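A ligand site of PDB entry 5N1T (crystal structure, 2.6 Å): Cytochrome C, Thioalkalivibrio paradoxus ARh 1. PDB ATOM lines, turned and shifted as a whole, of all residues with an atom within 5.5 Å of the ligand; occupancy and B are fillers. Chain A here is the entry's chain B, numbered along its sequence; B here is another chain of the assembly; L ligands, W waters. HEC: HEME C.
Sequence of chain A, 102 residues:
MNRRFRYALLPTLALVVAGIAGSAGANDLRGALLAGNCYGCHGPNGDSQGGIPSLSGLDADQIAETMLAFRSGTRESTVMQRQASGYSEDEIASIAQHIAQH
The side-chain sulfur (SG) of Cys 38 is covalently linked to a carbon (CAB) of the ligand, 1.6 Å away.
SG of Cys 41 is bonded to CAC of the ligand.
A ring nitrogen (NE2) of His 42 is bound to an iron atom (FE) of the ligand (1.9 Å).
N of Met 80 is in hydrogen-bond range of O2D of the ligand, 3.4 Å away.
FE of the ligand is bound by SD of Met 80, 2.3 Å away.
N of Thr 78 is in hydrogen-bond range of O2D of the ligand, at 3.0 Å.
OG1 of Thr 78 sits at hydrogen-bond distance from O1D of the ligand (2.4 Å).
NH2 of Arg 75 lies within salt-bridge range of O1A of the ligand (2.8 Å).
N of Val 79 lies within hydrogen-bond range of O2D of the ligand.
ND1 of His 42 is in hydrogen-bond range of O of Pro 53, at 2.9 Å.
The backbone NH of Met 80 is in hydrogen-bond range of the side-chain hydroxyl of Ser 77, 3.2 Å away.
OE1 of Gln 83 is in hydrogen-bond range of OG of Ser 365 of chain B, at 2.7 Å.
NE2 of Gln 83 lies within hydrogen-bond range of OG of Ser 381 of chain B (2.8 Å).
The side-chain hydroxyl of Thr 367 of chain B is in hydrogen-bond range of the side-chain hydroxyl of Ser 381 of chain B (2.9 Å).
O of Ile 63 lies within hydrogen-bond range of OG1 of Thr 66 (3.4 Å).
The side-chain hydroxyl (OG1) of Thr 66 is in hydrogen-bond range of the backbone carbonyl oxygen (O) of Gln 62 (2.8 Å).
Residues that only touch the ligand: Ser 77, Tyr 87, Phe 337 of chain B, Tyr 415 of chain B, Gln 83, Ile 95, Thr 367 of chain B, Ile 52, Leu 55, Phe 70, Thr 66, Met 67, Ile 63, Pro 53, Ile 99, Leu 34, Asn 37 and Tyr 369 of chain B.
Of the 33 residues printed, 25 come within 4 Å of the ligand.
The nearest printed residue that does not touch the ligand is Leu 58 (4.01 Å).
Water W1 bridges the side-chain amide oxygen (OE1) of Gln 83 (2.6 Å) and the side-chain hydroxyl (OH) of Tyr 87 (3.0 Å).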
ATOM      1  N   LEU A  34     -32.739 -16.818 -10.168  1.00  0.00           N
ATOM      2  CA  LEU A  34     -31.399 -16.872 -10.759  1.00  0.00           C
ATOM      3  C   LEU A  34     -31.508 -17.029 -12.255  1.00  0.00           C
ATOM      4  O   LEU A  34     -30.739 -16.399 -12.995  1.00  0.00           O
ATOM      5  CB  LEU A  34     -30.536 -17.997 -10.176  1.00  0.00           C
ATOM      6  CG  LEU A  34     -30.035 -17.804  -8.746  1.00  0.00           C
ATOM      7  CD1 LEU A  34     -29.529 -19.143  -8.244  1.00  0.00           C
ATOM      8  CD2 LEU A  34     -28.964 -16.725  -8.573  1.00  0.00           C
ATOM      9  N   ALA A  35     -32.492 -17.824 -12.672  1.00  0.00           N
ATOM     10  CA  ALA A  35     -32.680 -18.178 -14.068  1.00  0.00           C
ATOM     11  C   ALA A  35     -33.536 -17.165 -14.850  1.00  0.00           C
ATOM     12  O   ALA A  35     -33.231 -16.856 -16.011  1.00  0.00           O
ATOM     13  CB  ALA A  35     -33.283 -19.567 -14.160  1.00  0.00           C
ATOM     14  N   ASN A  37     -33.850 -14.048 -15.237  1.00  0.00           N
ATOM     15  CA  ASN A  37     -33.177 -12.945 -15.886  1.00  0.00           C
ATOM     16  C   ASN A  37     -32.598 -13.330 -17.238  1.00  0.00           C
ATOM     17  O   ASN A  37     -32.518 -12.493 -18.150  1.00  0.00           O
ATOM     18  CB  ASN A  37     -32.142 -12.344 -14.933  1.00  0.00           C
ATOM     19  CG  ASN A  37     -32.786 -11.480 -13.850  1.00  0.00           C
ATOM     20  OD1 ASN A  37     -33.435 -10.473 -14.144  1.00  0.00           O
ATOM     21  ND2 ASN A  37     -32.610 -11.861 -12.591  1.00  0.00           N
ATOM     22  N   CYS A  38     -32.247 -14.588 -17.395  1.00  0.00           N
ATOM     23  CA  CYS A  38     -31.743 -15.090 -18.682  1.00  0.00           C
ATOM     24  C   CYS A  38     -32.786 -14.968 -19.761  1.00  0.00           C
ATOM     25  O   CYS A  38     -32.453 -14.745 -20.920  1.00  0.00           O
ATOM     26  CB  CYS A  38     -31.317 -16.554 -18.580  1.00  0.00           C
ATOM     27  SG  CYS A  38     -30.273 -16.876 -17.151  1.00  0.00           S
ATOM     28  N   CYS A  41     -32.997 -11.538 -21.971  1.00  0.00           N
ATOM     29  CA  CYS A  41     -32.369 -11.489 -23.316  1.00  0.00           C
ATOM     30  C   CYS A  41     -32.666 -12.692 -24.190  1.00  0.00           C
ATOM     31  O   CYS A  41     -32.747 -12.555 -25.411  1.00  0.00           O
ATOM     32  CB  CYS A  41     -30.852 -11.412 -23.269  1.00  0.00           C
ATOM     33  SG  CYS A  41     -30.052  -9.949 -22.577  1.00  0.00           S
ATOM     34  N   HIS A  42     -32.761 -13.881 -23.573  1.00  0.00           N
ATOM     35  CA  HIS A  42     -32.802 -15.131 -24.333  1.00  0.00           C
ATOM     36  C   HIS A  42     -34.245 -15.514 -24.750  1.00  0.00           C
ATOM     37  O   HIS A  42     -34.438 -16.470 -25.505  1.00  0.00           O
ATOM     38  CB  HIS A  42     -32.027 -16.280 -23.626  1.00  0.00           C
ATOM     39  CG  HIS A  42     -30.527 -16.206 -23.762  1.00  0.00           C
ATOM     40  ND1 HIS A  42     -29.851 -16.607 -24.903  1.00  0.00           N
ATOM     41  CD2 HIS A  42     -29.553 -15.843 -22.875  1.00  0.00           C
ATOM     42  CE1 HIS A  42     -28.548 -16.460 -24.738  1.00  0.00           C
ATOM     43  NE2 HIS A  42     -28.339 -15.990 -23.515  1.00  0.00           N
ATOM     44  N   ILE A  52     -29.949 -13.082 -30.566  1.00  0.00           N
ATOM     45  CA  ILE A  52     -29.361 -13.738 -29.414  1.00  0.00           C
ATOM     46  C   ILE A  52     -29.754 -15.210 -29.606  1.00  0.00           C
ATOM     47  O   ILE A  52     -30.899 -15.485 -29.968  1.00  0.00           O
ATOM     48  CB  ILE A  52     -29.849 -13.120 -28.050  1.00  0.00           C
ATOM     49  CG1 ILE A  52     -29.583 -11.582 -27.981  1.00  0.00           C
ATOM     50  CG2 ILE A  52     -29.181 -13.804 -26.862  1.00  0.00           C
ATOM     51  CD1 ILE A  52     -30.062 -10.868 -26.724  1.00  0.00           C
ATOM     52  N   PRO A  53     -28.810 -16.159 -29.446  1.00  0.00           N
ATOM     53  CA  PRO A  53     -29.221 -17.563 -29.640  1.00  0.00           C
ATOM     54  C   PRO A  53     -30.255 -18.042 -28.609  1.00  0.00           C
ATOM     55  O   PRO A  53     -30.496 -17.349 -27.591  1.00  0.00           O
ATOM     56  CB  PRO A  53     -27.901 -18.339 -29.545  1.00  0.00           C
ATOM     57  CG  PRO A  53     -26.976 -17.439 -28.820  1.00  0.00           C
ATOM     58  CD  PRO A  53     -27.364 -16.046 -29.220  1.00  0.00           C
ATOM     59  N   SER A  54     -30.894 -19.173 -28.942  1.00  0.00           N
ATOM     60  CA  SER A  54     -31.940 -19.819 -28.118  1.00  0.00           C
ATOM     61  C   SER A  54     -31.308 -20.597 -26.965  1.00  0.00           C
ATOM     62  O   SER A  54     -30.109 -20.884 -26.961  1.00  0.00           O
ATOM     63  CB  SER A  54     -32.824 -20.773 -28.948  1.00  0.00           C
ATOM     64  OG  SER A  54     -33.768 -20.070 -29.724  1.00  0.00           O
ATOM     65  N   LEU A  55     -32.118 -20.945 -25.969  1.00  0.00           N
ATOM     66  CA  LEU A  55     -31.562 -21.583 -24.794  1.00  0.00           C
ATOM     67  C   LEU A  55     -32.208 -22.948 -24.556  1.00  0.00           C
ATOM     68  O   LEU A  55     -31.539 -23.905 -24.155  1.00  0.00           O
ATOM     69  CB  LEU A  55     -31.724 -20.646 -23.602  1.00  0.00           C
ATOM     70  CG  LEU A  55     -30.475 -20.426 -22.771  1.00  0.00           C
ATOM     71  CD1 LEU A  55     -29.380 -19.812 -23.638  1.00  0.00           C
ATOM     72  CD2 LEU A  55     -30.753 -19.593 -21.517  1.00  0.00           C
ATOM     73  N   LEU A  58     -31.066 -27.101 -25.075  1.00  0.00           N
ATOM     74  CA  LEU A  58     -29.752 -27.287 -24.453  1.00  0.00           C
ATOM     75  C   LEU A  58     -29.981 -27.900 -23.088  1.00  0.00           C
ATOM     76  O   LEU A  58     -30.962 -27.564 -22.412  1.00  0.00           O
ATOM     77  CB  LEU A  58     -29.059 -25.938 -24.213  1.00  0.00           C
ATOM     78  CG  LEU A  58     -28.315 -25.098 -25.268  1.00  0.00           C
ATOM     79  CD1 LEU A  58     -27.580 -23.932 -24.603  1.00  0.00           C
ATOM     80  CD2 LEU A  58     -27.315 -25.943 -26.040  1.00  0.00           C
ATOM     81  N   GLN A  62     -24.415 -28.508 -20.863  1.00  0.00           N
ATOM     82  CA  GLN A  62     -24.030 -27.509 -21.881  1.00  0.00           C
ATOM     83  C   GLN A  62     -24.078 -26.083 -21.347  1.00  0.00           C
ATOM     84  O   GLN A  62     -23.107 -25.320 -21.504  1.00  0.00           O
ATOM     85  CB  GLN A  62     -24.914 -27.605 -23.122  1.00  0.00           C
ATOM     86  CG  GLN A  62     -24.801 -28.925 -23.859  1.00  0.00           C
ATOM     87  CD  GLN A  62     -25.935 -29.118 -24.825  1.00  0.00           C
ATOM     88  OE1 GLN A  62     -27.096 -29.226 -24.442  1.00  0.00           O
ATOM     89  NE2 GLN A  62     -25.600 -29.157 -26.108  1.00  0.00           N
ATOM     90  N   ILE A  63     -25.191 -25.755 -20.692  1.00  0.00           N
ATOM     91  CA  ILE A  63     -25.350 -24.417 -20.145  1.00  0.00           C
ATOM     92  C   ILE A  63     -24.240 -24.159 -19.141  1.00  0.00           C
ATOM     93  O   ILE A  63     -23.468 -23.224 -19.326  1.00  0.00           O
ATOM     94  CB  ILE A  63     -26.741 -24.154 -19.549  1.00  0.00           C
ATOM     95  CG1 ILE A  63     -27.817 -24.203 -20.668  1.00  0.00           C
ATOM     96  CG2 ILE A  63     -26.720 -22.802 -18.818  1.00  0.00           C
ATOM     97  CD1 ILE A  63     -29.283 -24.239 -20.203  1.00  0.00           C
ATOM     98  N   THR A  66     -20.594 -23.815 -20.541  1.00  0.00           N
ATOM     99  CA  THR A  66     -20.320 -22.578 -21.318  1.00  0.00           C
ATOM    100  C   THR A  66     -20.481 -21.260 -20.556  1.00  0.00           C
ATOM    101  O   THR A  66     -19.764 -20.303 -20.846  1.00  0.00           O
ATOM    102  CB  THR A  66     -20.999 -22.537 -22.710  1.00  0.00           C
ATOM    103  OG1 THR A  66     -22.390 -22.847 -22.573  1.00  0.00           O
ATOM    104  CG2 THR A  66     -20.325 -23.545 -23.671  1.00  0.00           C
ATOM    105  N   MET A  67     -21.364 -21.243 -19.561  1.00  0.00           N
ATOM    106  CA  MET A  67     -21.384 -20.175 -18.558  1.00  0.00           C
ATOM    107  C   MET A  67     -19.973 -19.977 -18.053  1.00  0.00           C
ATOM    108  O   MET A  67     -19.391 -18.902 -18.205  1.00  0.00           O
ATOM    109  CB  MET A  67     -22.301 -20.514 -17.383  1.00  0.00           C
ATOM    110  CG  MET A  67     -23.780 -20.442 -17.667  1.00  0.00           C
ATOM    111  SD  MET A  67     -24.263 -18.754 -17.983  1.00  0.00           S
ATOM    112  CE  MET A  67     -24.756 -18.248 -16.338  1.00  0.00           C
ATOM    113  N   PHE A  70     -17.487 -18.710 -20.606  1.00  0.00           N
ATOM    114  CA  PHE A  70     -17.636 -17.285 -20.837  1.00  0.00           C
ATOM    115  C   PHE A  70     -17.020 -16.538 -19.666  1.00  0.00           C
ATOM    116  O   PHE A  70     -16.262 -15.565 -19.860  1.00  0.00           O
ATOM    117  CB  PHE A  70     -19.116 -16.908 -20.944  1.00  0.00           C
ATOM    118  CG  PHE A  70     -19.738 -17.163 -22.292  1.00  0.00           C
ATOM    119  CD1 PHE A  70     -19.114 -16.765 -23.472  1.00  0.00           C
ATOM    120  CD2 PHE A  70     -21.004 -17.760 -22.380  1.00  0.00           C
ATOM    121  CE1 PHE A  70     -19.728 -16.975 -24.708  1.00  0.00           C
ATOM    122  CE2 PHE A  70     -21.622 -17.973 -23.607  1.00  0.00           C
ATOM    123  CZ  PHE A  70     -20.996 -17.586 -24.778  1.00  0.00           C
ATOM    124  N   ARG A  75     -14.219 -18.822 -23.776  1.00  0.00           N
ATOM    125  CA  ARG A  75     -15.164 -18.510 -24.816  1.00  0.00           C
ATOM    126  C   ARG A  75     -15.405 -16.972 -24.774  1.00  0.00           C
ATOM    127  O   ARG A  75     -15.832 -16.425 -23.731  1.00  0.00           O
ATOM    128  CB  ARG A  75     -16.434 -19.330 -24.615  1.00  0.00           C
ATOM    129  CG  ARG A  75     -16.954 -19.893 -25.905  1.00  0.00           C
ATOM    130  CD  ARG A  75     -18.212 -20.676 -25.691  1.00  0.00           C
ATOM    131  NE  ARG A  75     -19.162 -20.300 -26.730  1.00  0.00           N
ATOM    132  CZ  ARG A  75     -20.209 -21.015 -27.120  1.00  0.00           C
ATOM    133  NH1 ARG A  75     -20.483 -22.199 -26.584  1.00  0.00           N
ATOM    134  NH2 ARG A  75     -20.984 -20.545 -28.091  1.00  0.00           N
ATOM    135  N   GLU A  76     -15.055 -16.320 -25.883  1.00  0.00           N
ATOM    136  CA  GLU A  76     -15.200 -14.860 -26.106  1.00  0.00           C
ATOM    137  C   GLU A  76     -16.671 -14.461 -26.082  1.00  0.00           C
ATOM    138  O   GLU A  76     -17.502 -15.129 -26.728  1.00  0.00           O
ATOM    139  CB  GLU A  76     -14.608 -14.493 -27.481  1.00  0.00           C
ATOM    140  CG  GLU A  76     -13.102 -14.673 -27.584  1.00  0.00           C
ATOM    141  CD  GLU A  76     -12.351 -13.472 -27.058  1.00  0.00           C
ATOM    142  OE1 GLU A  76     -12.223 -12.474 -27.804  1.00  0.00           O
ATOM    143  OE2 GLU A  76     -11.907 -13.531 -25.884  1.00  0.00           O
ATOM    144  N   SER A  77     -17.022 -13.400 -25.355  1.00  0.00           N
ATOM    145  CA  SER A  77     -18.416 -12.917 -25.392  1.00  0.00           C
ATOM    146  C   SER A  77     -18.487 -11.449 -25.770  1.00  0.00           C
ATOM    147  O   SER A  77     -17.493 -10.739 -25.655  1.00  0.00           O
ATOM    148  CB  SER A  77     -19.108 -13.164 -24.051  1.00  0.00           C
ATOM    149  OG  SER A  77     -18.601 -12.320 -23.044  1.00  0.00           O
ATOM    150  N   THR A  78     -19.647 -11.004 -26.262  1.00  0.00           N
ATOM    151  CA  THR A  78     -19.943  -9.568 -26.307  1.00  0.00           C
ATOM    152  C   THR A  78     -20.453  -9.082 -24.971  1.00  0.00           C
ATOM    153  O   THR A  78     -20.124  -7.992 -24.561  1.00  0.00           O
ATOM    154  CB  THR A  78     -20.946  -9.138 -27.389  1.00  0.00           C
ATOM    155  OG1 THR A  78     -21.945 -10.149 -27.552  1.00  0.00           O
ATOM    156  CG2 THR A  78     -20.243  -8.931 -28.690  1.00  0.00           C
ATOM    157  N   VAL A  79     -21.247  -9.900 -24.295  1.00  0.00           N
ATOM    158  CA  VAL A  79     -21.836  -9.541 -22.996  1.00  0.00           C
ATOM    159  C   VAL A  79     -21.923 -10.705 -22.007  1.00  0.00           C
ATOM    160  O   VAL A  79     -22.133 -10.492 -20.822  1.00  0.00           O
ATOM    161  CB  VAL A  79     -23.231  -8.908 -23.197  1.00  0.00           C
ATOM    162  CG1 VAL A  79     -24.271  -9.964 -23.596  1.00  0.00           C
ATOM    163  CG2 VAL A  79     -23.629  -8.097 -21.974  1.00  0.00           C
ATOM    164  N   MET A  80     -21.752 -11.939 -22.504  1.00  0.00           N
ATOM    165  CA  MET A  80     -21.902 -13.097 -21.638  1.00  0.00           C
ATOM    166  C   MET A  80     -20.961 -13.216 -20.456  1.00  0.00           C
ATOM    167  O   MET A  80     -21.385 -13.679 -19.399  1.00  0.00           O
ATOM    168  CB  MET A  80     -22.023 -14.408 -22.400  1.00  0.00           C
ATOM    169  CG  MET A  80     -23.447 -14.702 -22.889  1.00  0.00           C
ATOM    170  SD  MET A  80     -24.806 -14.856 -21.682  1.00  0.00           S
ATOM    171  CE  MET A  80     -24.127 -15.926 -20.423  1.00  0.00           C
ATOM    172  N   GLN A  83     -22.228 -10.899 -17.720  1.00  0.00           N
ATOM    173  CA  GLN A  83     -23.334 -11.546 -17.041  1.00  0.00           C
ATOM    174  C   GLN A  83     -22.854 -12.754 -16.222  1.00  0.00           C
ATOM    175  O   GLN A  83     -23.039 -12.785 -15.005  1.00  0.00           O
ATOM    176  CB  GLN A  83     -24.411 -11.932 -18.061  1.00  0.00           C
ATOM    177  CG  GLN A  83     -25.318 -10.799 -18.539  1.00  0.00           C
ATOM    178  CD  GLN A  83     -26.146 -10.249 -17.401  1.00  0.00           C
ATOM    179  OE1 GLN A  83     -26.909 -10.972 -16.779  1.00  0.00           O
ATOM    180  NE2 GLN A  83     -25.968  -8.950 -17.103  1.00  0.00           N
ATOM    181  N   TYR A  87     -22.313 -14.445 -11.432  1.00  0.00           N
ATOM    182  CA  TYR A  87     -22.721 -15.623 -10.684  1.00  0.00           C
ATOM    183  C   TYR A  87     -21.579 -16.478 -10.160  1.00  0.00           C
ATOM    184  O   TYR A  87     -20.520 -16.579 -10.774  1.00  0.00           O
ATOM    185  CB  TYR A  87     -23.613 -16.481 -11.539  1.00  0.00           C
ATOM    186  CG  TYR A  87     -24.762 -15.739 -12.113  1.00  0.00           C
ATOM    187  CD1 TYR A  87     -25.879 -15.429 -11.310  1.00  0.00           C
ATOM    188  CD2 TYR A  87     -24.741 -15.328 -13.430  1.00  0.00           C
ATOM    189  CE1 TYR A  87     -26.955 -14.742 -11.834  1.00  0.00           C
ATOM    190  CE2 TYR A  87     -25.808 -14.637 -13.950  1.00  0.00           C
ATOM    191  CZ  TYR A  87     -26.905 -14.350 -13.166  1.00  0.00           C
ATOM    192  OH  TYR A  87     -27.974 -13.670 -13.722  1.00  0.00           O
ATOM    193  N   ILE A  95     -28.881 -22.429 -12.181  1.00  0.00           N
ATOM    194  CA  ILE A  95     -29.390 -21.789 -13.404  1.00  0.00           C
ATOM    195  C   ILE A  95     -29.450 -22.825 -14.519  1.00  0.00           C
ATOM    196  O   ILE A  95     -30.468 -22.948 -15.226  1.00  0.00           O
ATOM    197  CB  ILE A  95     -28.497 -20.588 -13.811  1.00  0.00           C
ATOM    198  CG1 ILE A  95     -28.735 -19.424 -12.873  1.00  0.00           C
ATOM    199  CG2 ILE A  95     -28.745 -20.103 -15.240  1.00  0.00           C
ATOM    200  CD1 ILE A  95     -27.481 -18.590 -12.693  1.00  0.00           C
ATOM    201  N   ILE A  99     -33.109 -24.090 -16.245  1.00  0.00           N
ATOM    202  CA  ILE A  99     -33.460 -23.801 -17.650  1.00  0.00           C
ATOM    203  C   ILE A  99     -33.748 -25.079 -18.448  1.00  0.00           C
ATOM    204  O   ILE A  99     -34.789 -25.161 -19.100  1.00  0.00           O
ATOM    205  CB  ILE A  99     -32.471 -22.821 -18.333  1.00  0.00           C
ATOM    206  CG1 ILE A  99     -32.638 -21.422 -17.731  1.00  0.00           C
ATOM    207  CG2 ILE A  99     -32.710 -22.741 -19.839  1.00  0.00           C
ATOM    208  CD1 ILE A  99     -31.385 -20.568 -17.832  1.00  0.00           C
ATOM    209  N   PHE B 337     -35.105  -3.135 -18.358  1.00  0.00           N
ATOM    210  CA  PHE B 337     -34.585  -4.452 -17.977  1.00  0.00           C
ATOM    211  C   PHE B 337     -34.671  -4.590 -16.470  1.00  0.00           C
ATOM    212  O   PHE B 337     -35.057  -5.639 -15.959  1.00  0.00           O
ATOM    213  CB  PHE B 337     -33.135  -4.602 -18.458  1.00  0.00           C
ATOM    214  CG  PHE B 337     -32.754  -6.004 -18.855  1.00  0.00           C
ATOM    215  CD1 PHE B 337     -33.142  -7.140 -18.089  1.00  0.00           C
ATOM    216  CD2 PHE B 337     -31.937  -6.215 -19.996  1.00  0.00           C
ATOM    217  CE1 PHE B 337     -32.768  -8.457 -18.480  1.00  0.00           C
ATOM    218  CE2 PHE B 337     -31.571  -7.525 -20.378  1.00  0.00           C
ATOM    219  CZ  PHE B 337     -31.993  -8.643 -19.633  1.00  0.00           C
ATOM    220  N   SER B 365     -30.705  -8.579 -12.721  1.00  0.00           N
ATOM    221  CA  SER B 365     -29.765  -8.267 -13.772  1.00  0.00           C
ATOM    222  C   SER B 365     -30.302  -7.057 -14.503  1.00  0.00           C
ATOM    223  O   SER B 365     -31.496  -6.887 -14.576  1.00  0.00           O
ATOM    224  CB  SER B 365     -29.563  -9.470 -14.723  1.00  0.00           C
ATOM    225  OG  SER B 365     -28.720  -9.147 -15.832  1.00  0.00           O
ATOM    226  N   THR B 367     -29.290  -4.586 -18.161  1.00  0.00           N
ATOM    227  CA  THR B 367     -28.427  -4.330 -19.321  1.00  0.00           C
ATOM    228  C   THR B 367     -29.083  -3.284 -20.169  1.00  0.00           C
ATOM    229  O   THR B 367     -30.233  -3.459 -20.588  1.00  0.00           O
ATOM    230  CB  THR B 367     -28.209  -5.607 -20.139  1.00  0.00           C
ATOM    231  OG1 THR B 367     -27.829  -6.687 -19.265  1.00  0.00           O
ATOM    232  CG2 THR B 367     -27.179  -5.372 -21.249  1.00  0.00           C
ATOM    233  N   TYR B 369     -28.713  -1.565 -23.614  1.00  0.00           N
ATOM    234  CA  TYR B 369     -28.153  -1.481 -24.977  1.00  0.00           C
ATOM    235  C   TYR B 369     -28.495  -0.158 -25.595  1.00  0.00           C
ATOM    236  O   TYR B 369     -29.666   0.284 -25.509  1.00  0.00           O
ATOM    237  CB  TYR B 369     -28.762  -2.520 -25.937  1.00  0.00           C
ATOM    238  CG  TYR B 369     -28.257  -3.959 -25.799  1.00  0.00           C
ATOM    239  CD1 TYR B 369     -27.148  -4.388 -26.500  1.00  0.00           C
ATOM    240  CD2 TYR B 369     -28.944  -4.886 -24.994  1.00  0.00           C
ATOM    241  CE1 TYR B 369     -26.689  -5.682 -26.380  1.00  0.00           C
ATOM    242  CE2 TYR B 369     -28.502  -6.198 -24.874  1.00  0.00           C
ATOM    243  CZ  TYR B 369     -27.365  -6.580 -25.575  1.00  0.00           C
ATOM    244  OH  TYR B 369     -26.908  -7.852 -25.473  1.00  0.00           O
ATOM    245  N   SER B 381     -23.822  -3.518 -18.575  1.00  0.00           N
ATOM    246  CA  SER B 381     -24.505  -4.729 -18.141  1.00  0.00           C
ATOM    247  C   SER B 381     -24.040  -5.163 -16.758  1.00  0.00           C
ATOM    248  O   SER B 381     -22.848  -5.074 -16.463  1.00  0.00           O
ATOM    249  CB  SER B 381     -24.276  -5.862 -19.164  1.00  0.00           C
ATOM    250  OG  SER B 381     -25.011  -7.050 -18.866  1.00  0.00           O
ATOM    251  N   TYR B 415     -27.629  -7.860 -31.224  1.00  0.00           N
ATOM    252  CA  TYR B 415     -28.095  -8.373 -29.942  1.00  0.00           C
ATOM    253  C   TYR B 415     -29.081  -7.429 -29.240  1.00  0.00           C
ATOM    254  O   TYR B 415     -30.021  -7.907 -28.567  1.00  0.00           O
ATOM    255  CB  TYR B 415     -26.912  -8.799 -29.052  1.00  0.00           C
ATOM    256  CG  TYR B 415     -26.048  -9.893 -29.660  1.00  0.00           C
ATOM    257  CD1 TYR B 415     -26.612 -10.964 -30.368  1.00  0.00           C
ATOM    258  CD2 TYR B 415     -24.661  -9.850 -29.518  1.00  0.00           C
ATOM    259  CE1 TYR B 415     -25.806 -11.944 -30.940  1.00  0.00           C
ATOM    260  CE2 TYR B 415     -23.854 -10.830 -30.068  1.00  0.00           C
ATOM    261  CZ  TYR B 415     -24.414 -11.888 -30.771  1.00  0.00           C
ATOM    262  OH  TYR B 415     -23.574 -12.864 -31.296  1.00  0.00           O
ATOM    263  N   TRP B 419     -32.490  -8.630 -27.709  1.00  0.00           N
ATOM    264  CA  TRP B 419     -33.033  -8.203 -26.421  1.00  0.00           C
ATOM    265  C   TRP B 419     -34.433  -7.564 -26.568  1.00  0.00           C
ATOM    266  O   TRP B 419     -35.371  -7.941 -25.871  1.00  0.00           O
ATOM    267  CB  TRP B 419     -32.065  -7.237 -25.697  1.00  0.00           C
ATOM    268  CG  TRP B 419     -32.784  -6.523 -24.590  1.00  0.00           C
ATOM    269  CD1 TRP B 419     -33.150  -7.052 -23.393  1.00  0.00           C
ATOM    270  CD2 TRP B 419     -33.335  -5.198 -24.652  1.00  0.00           C
ATOM    271  NE1 TRP B 419     -33.870  -6.124 -22.677  1.00  0.00           N
ATOM    272  CE2 TRP B 419     -33.992  -4.980 -23.424  1.00  0.00           C
ATOM    273  CE3 TRP B 419     -33.316  -4.178 -25.612  1.00  0.00           C
ATOM    274  CZ2 TRP B 419     -34.621  -3.772 -23.125  1.00  0.00           C
ATOM    275  CZ3 TRP B 419     -33.923  -2.993 -25.311  1.00  0.00           C
ATOM    276  CH2 TRP B 419     -34.596  -2.794 -24.059  1.00  0.00           C
HETATM  277 FE   HEC L   1     -26.833 -15.416 -22.557  1.00  0.00          FE
HETATM  278  CHA HEC L   1     -24.987 -16.497 -25.301  1.00  0.00           C
HETATM  279  CHB HEC L   1     -26.868 -18.576 -21.340  1.00  0.00           C
HETATM  280  CHC HEC L   1     -28.124 -14.222 -19.524  1.00  0.00           C
HETATM  281  CHD HEC L   1     -27.175 -12.367 -23.960  1.00  0.00           C
HETATM  282  NA  HEC L   1     -26.038 -17.222 -23.211  1.00  0.00           N
HETATM  283  C1A HEC L   1     -25.369 -17.526 -24.333  1.00  0.00           C
HETATM  284  C2A HEC L   1     -24.994 -18.950 -24.506  1.00  0.00           C
HETATM  285  C3A HEC L   1     -25.554 -19.562 -23.306  1.00  0.00           C
HETATM  286  C4A HEC L   1     -26.150 -18.407 -22.611  1.00  0.00           C
HETATM  287  CMA HEC L   1     -25.533 -20.980 -22.827  1.00  0.00           C
HETATM  288  CAA HEC L   1     -24.254 -19.587 -25.654  1.00  0.00           C
HETATM  289  CBA HEC L   1     -25.394 -19.961 -26.609  1.00  0.00           C
HETATM  290  CGA HEC L   1     -24.985 -20.754 -27.846  1.00  0.00           C
HETATM  291  O1A HEC L   1     -23.795 -20.800 -28.219  1.00  0.00           O
HETATM  292  O2A HEC L   1     -25.880 -21.343 -28.487  1.00  0.00           O
HETATM  293  NB  HEC L   1     -27.389 -16.248 -20.724  1.00  0.00           N
HETATM  294  C1B HEC L   1     -27.347 -17.572 -20.423  1.00  0.00           C
HETATM  295  C2B HEC L   1     -27.813 -17.965 -19.081  1.00  0.00           C
HETATM  296  C3B HEC L   1     -28.162 -16.676 -18.499  1.00  0.00           C
HETATM  297  C4B HEC L   1     -27.883 -15.670 -19.602  1.00  0.00           C
HETATM  298  CMB HEC L   1     -27.865 -19.313 -18.428  1.00  0.00           C
HETATM  299  CAB HEC L   1     -28.654 -16.640 -17.093  1.00  0.00           C
HETATM  300  CBB HEC L   1     -29.059 -15.462 -16.294  1.00  0.00           C
HETATM  301  NC  HEC L   1     -27.555 -13.590 -21.849  1.00  0.00           N
HETATM  302  C1C HEC L   1     -28.074 -13.260 -20.639  1.00  0.00           C
HETATM  303  C2C HEC L   1     -28.517 -11.834 -20.503  1.00  0.00           C
HETATM  304  C3C HEC L   1     -28.198 -11.300 -21.850  1.00  0.00           C
HETATM  305  C4C HEC L   1     -27.635 -12.459 -22.570  1.00  0.00           C
HETATM  306  CMC HEC L   1     -29.115 -11.175 -19.294  1.00  0.00           C
HETATM  307  CAC HEC L   1     -28.380  -9.976 -22.524  1.00  0.00           C
HETATM  308  CBC HEC L   1     -28.876  -8.737 -21.891  1.00  0.00           C
HETATM  309  ND  HEC L   1     -26.178 -14.584 -24.319  1.00  0.00           N
HETATM  310  C1D HEC L   1     -26.358 -13.324 -24.721  1.00  0.00           C
HETATM  311  C2D HEC L   1     -25.737 -12.990 -26.027  1.00  0.00           C
HETATM  312  C3D HEC L   1     -25.095 -14.255 -26.420  1.00  0.00           C
HETATM  313  C4D HEC L   1     -25.438 -15.126 -25.291  1.00  0.00           C
HETATM  314  CMD HEC L   1     -25.779 -11.717 -26.789  1.00  0.00           C
HETATM  315  CAD HEC L   1     -24.277 -14.586 -27.622  1.00  0.00           C
HETATM  316  CBD HEC L   1     -22.857 -14.596 -27.061  1.00  0.00           C
HETATM  317  CGD HEC L   1     -22.206 -13.230 -26.922  1.00  0.00           C
HETATM  318  O1D HEC L   1     -21.954 -12.562 -27.947  1.00  0.00           O
HETATM  319  O2D HEC L   1     -21.911 -12.838 -25.772  1.00  0.00           O
HETATM  320  O   HOH W   1     -28.843 -12.643 -16.396  1.00  0.00           O
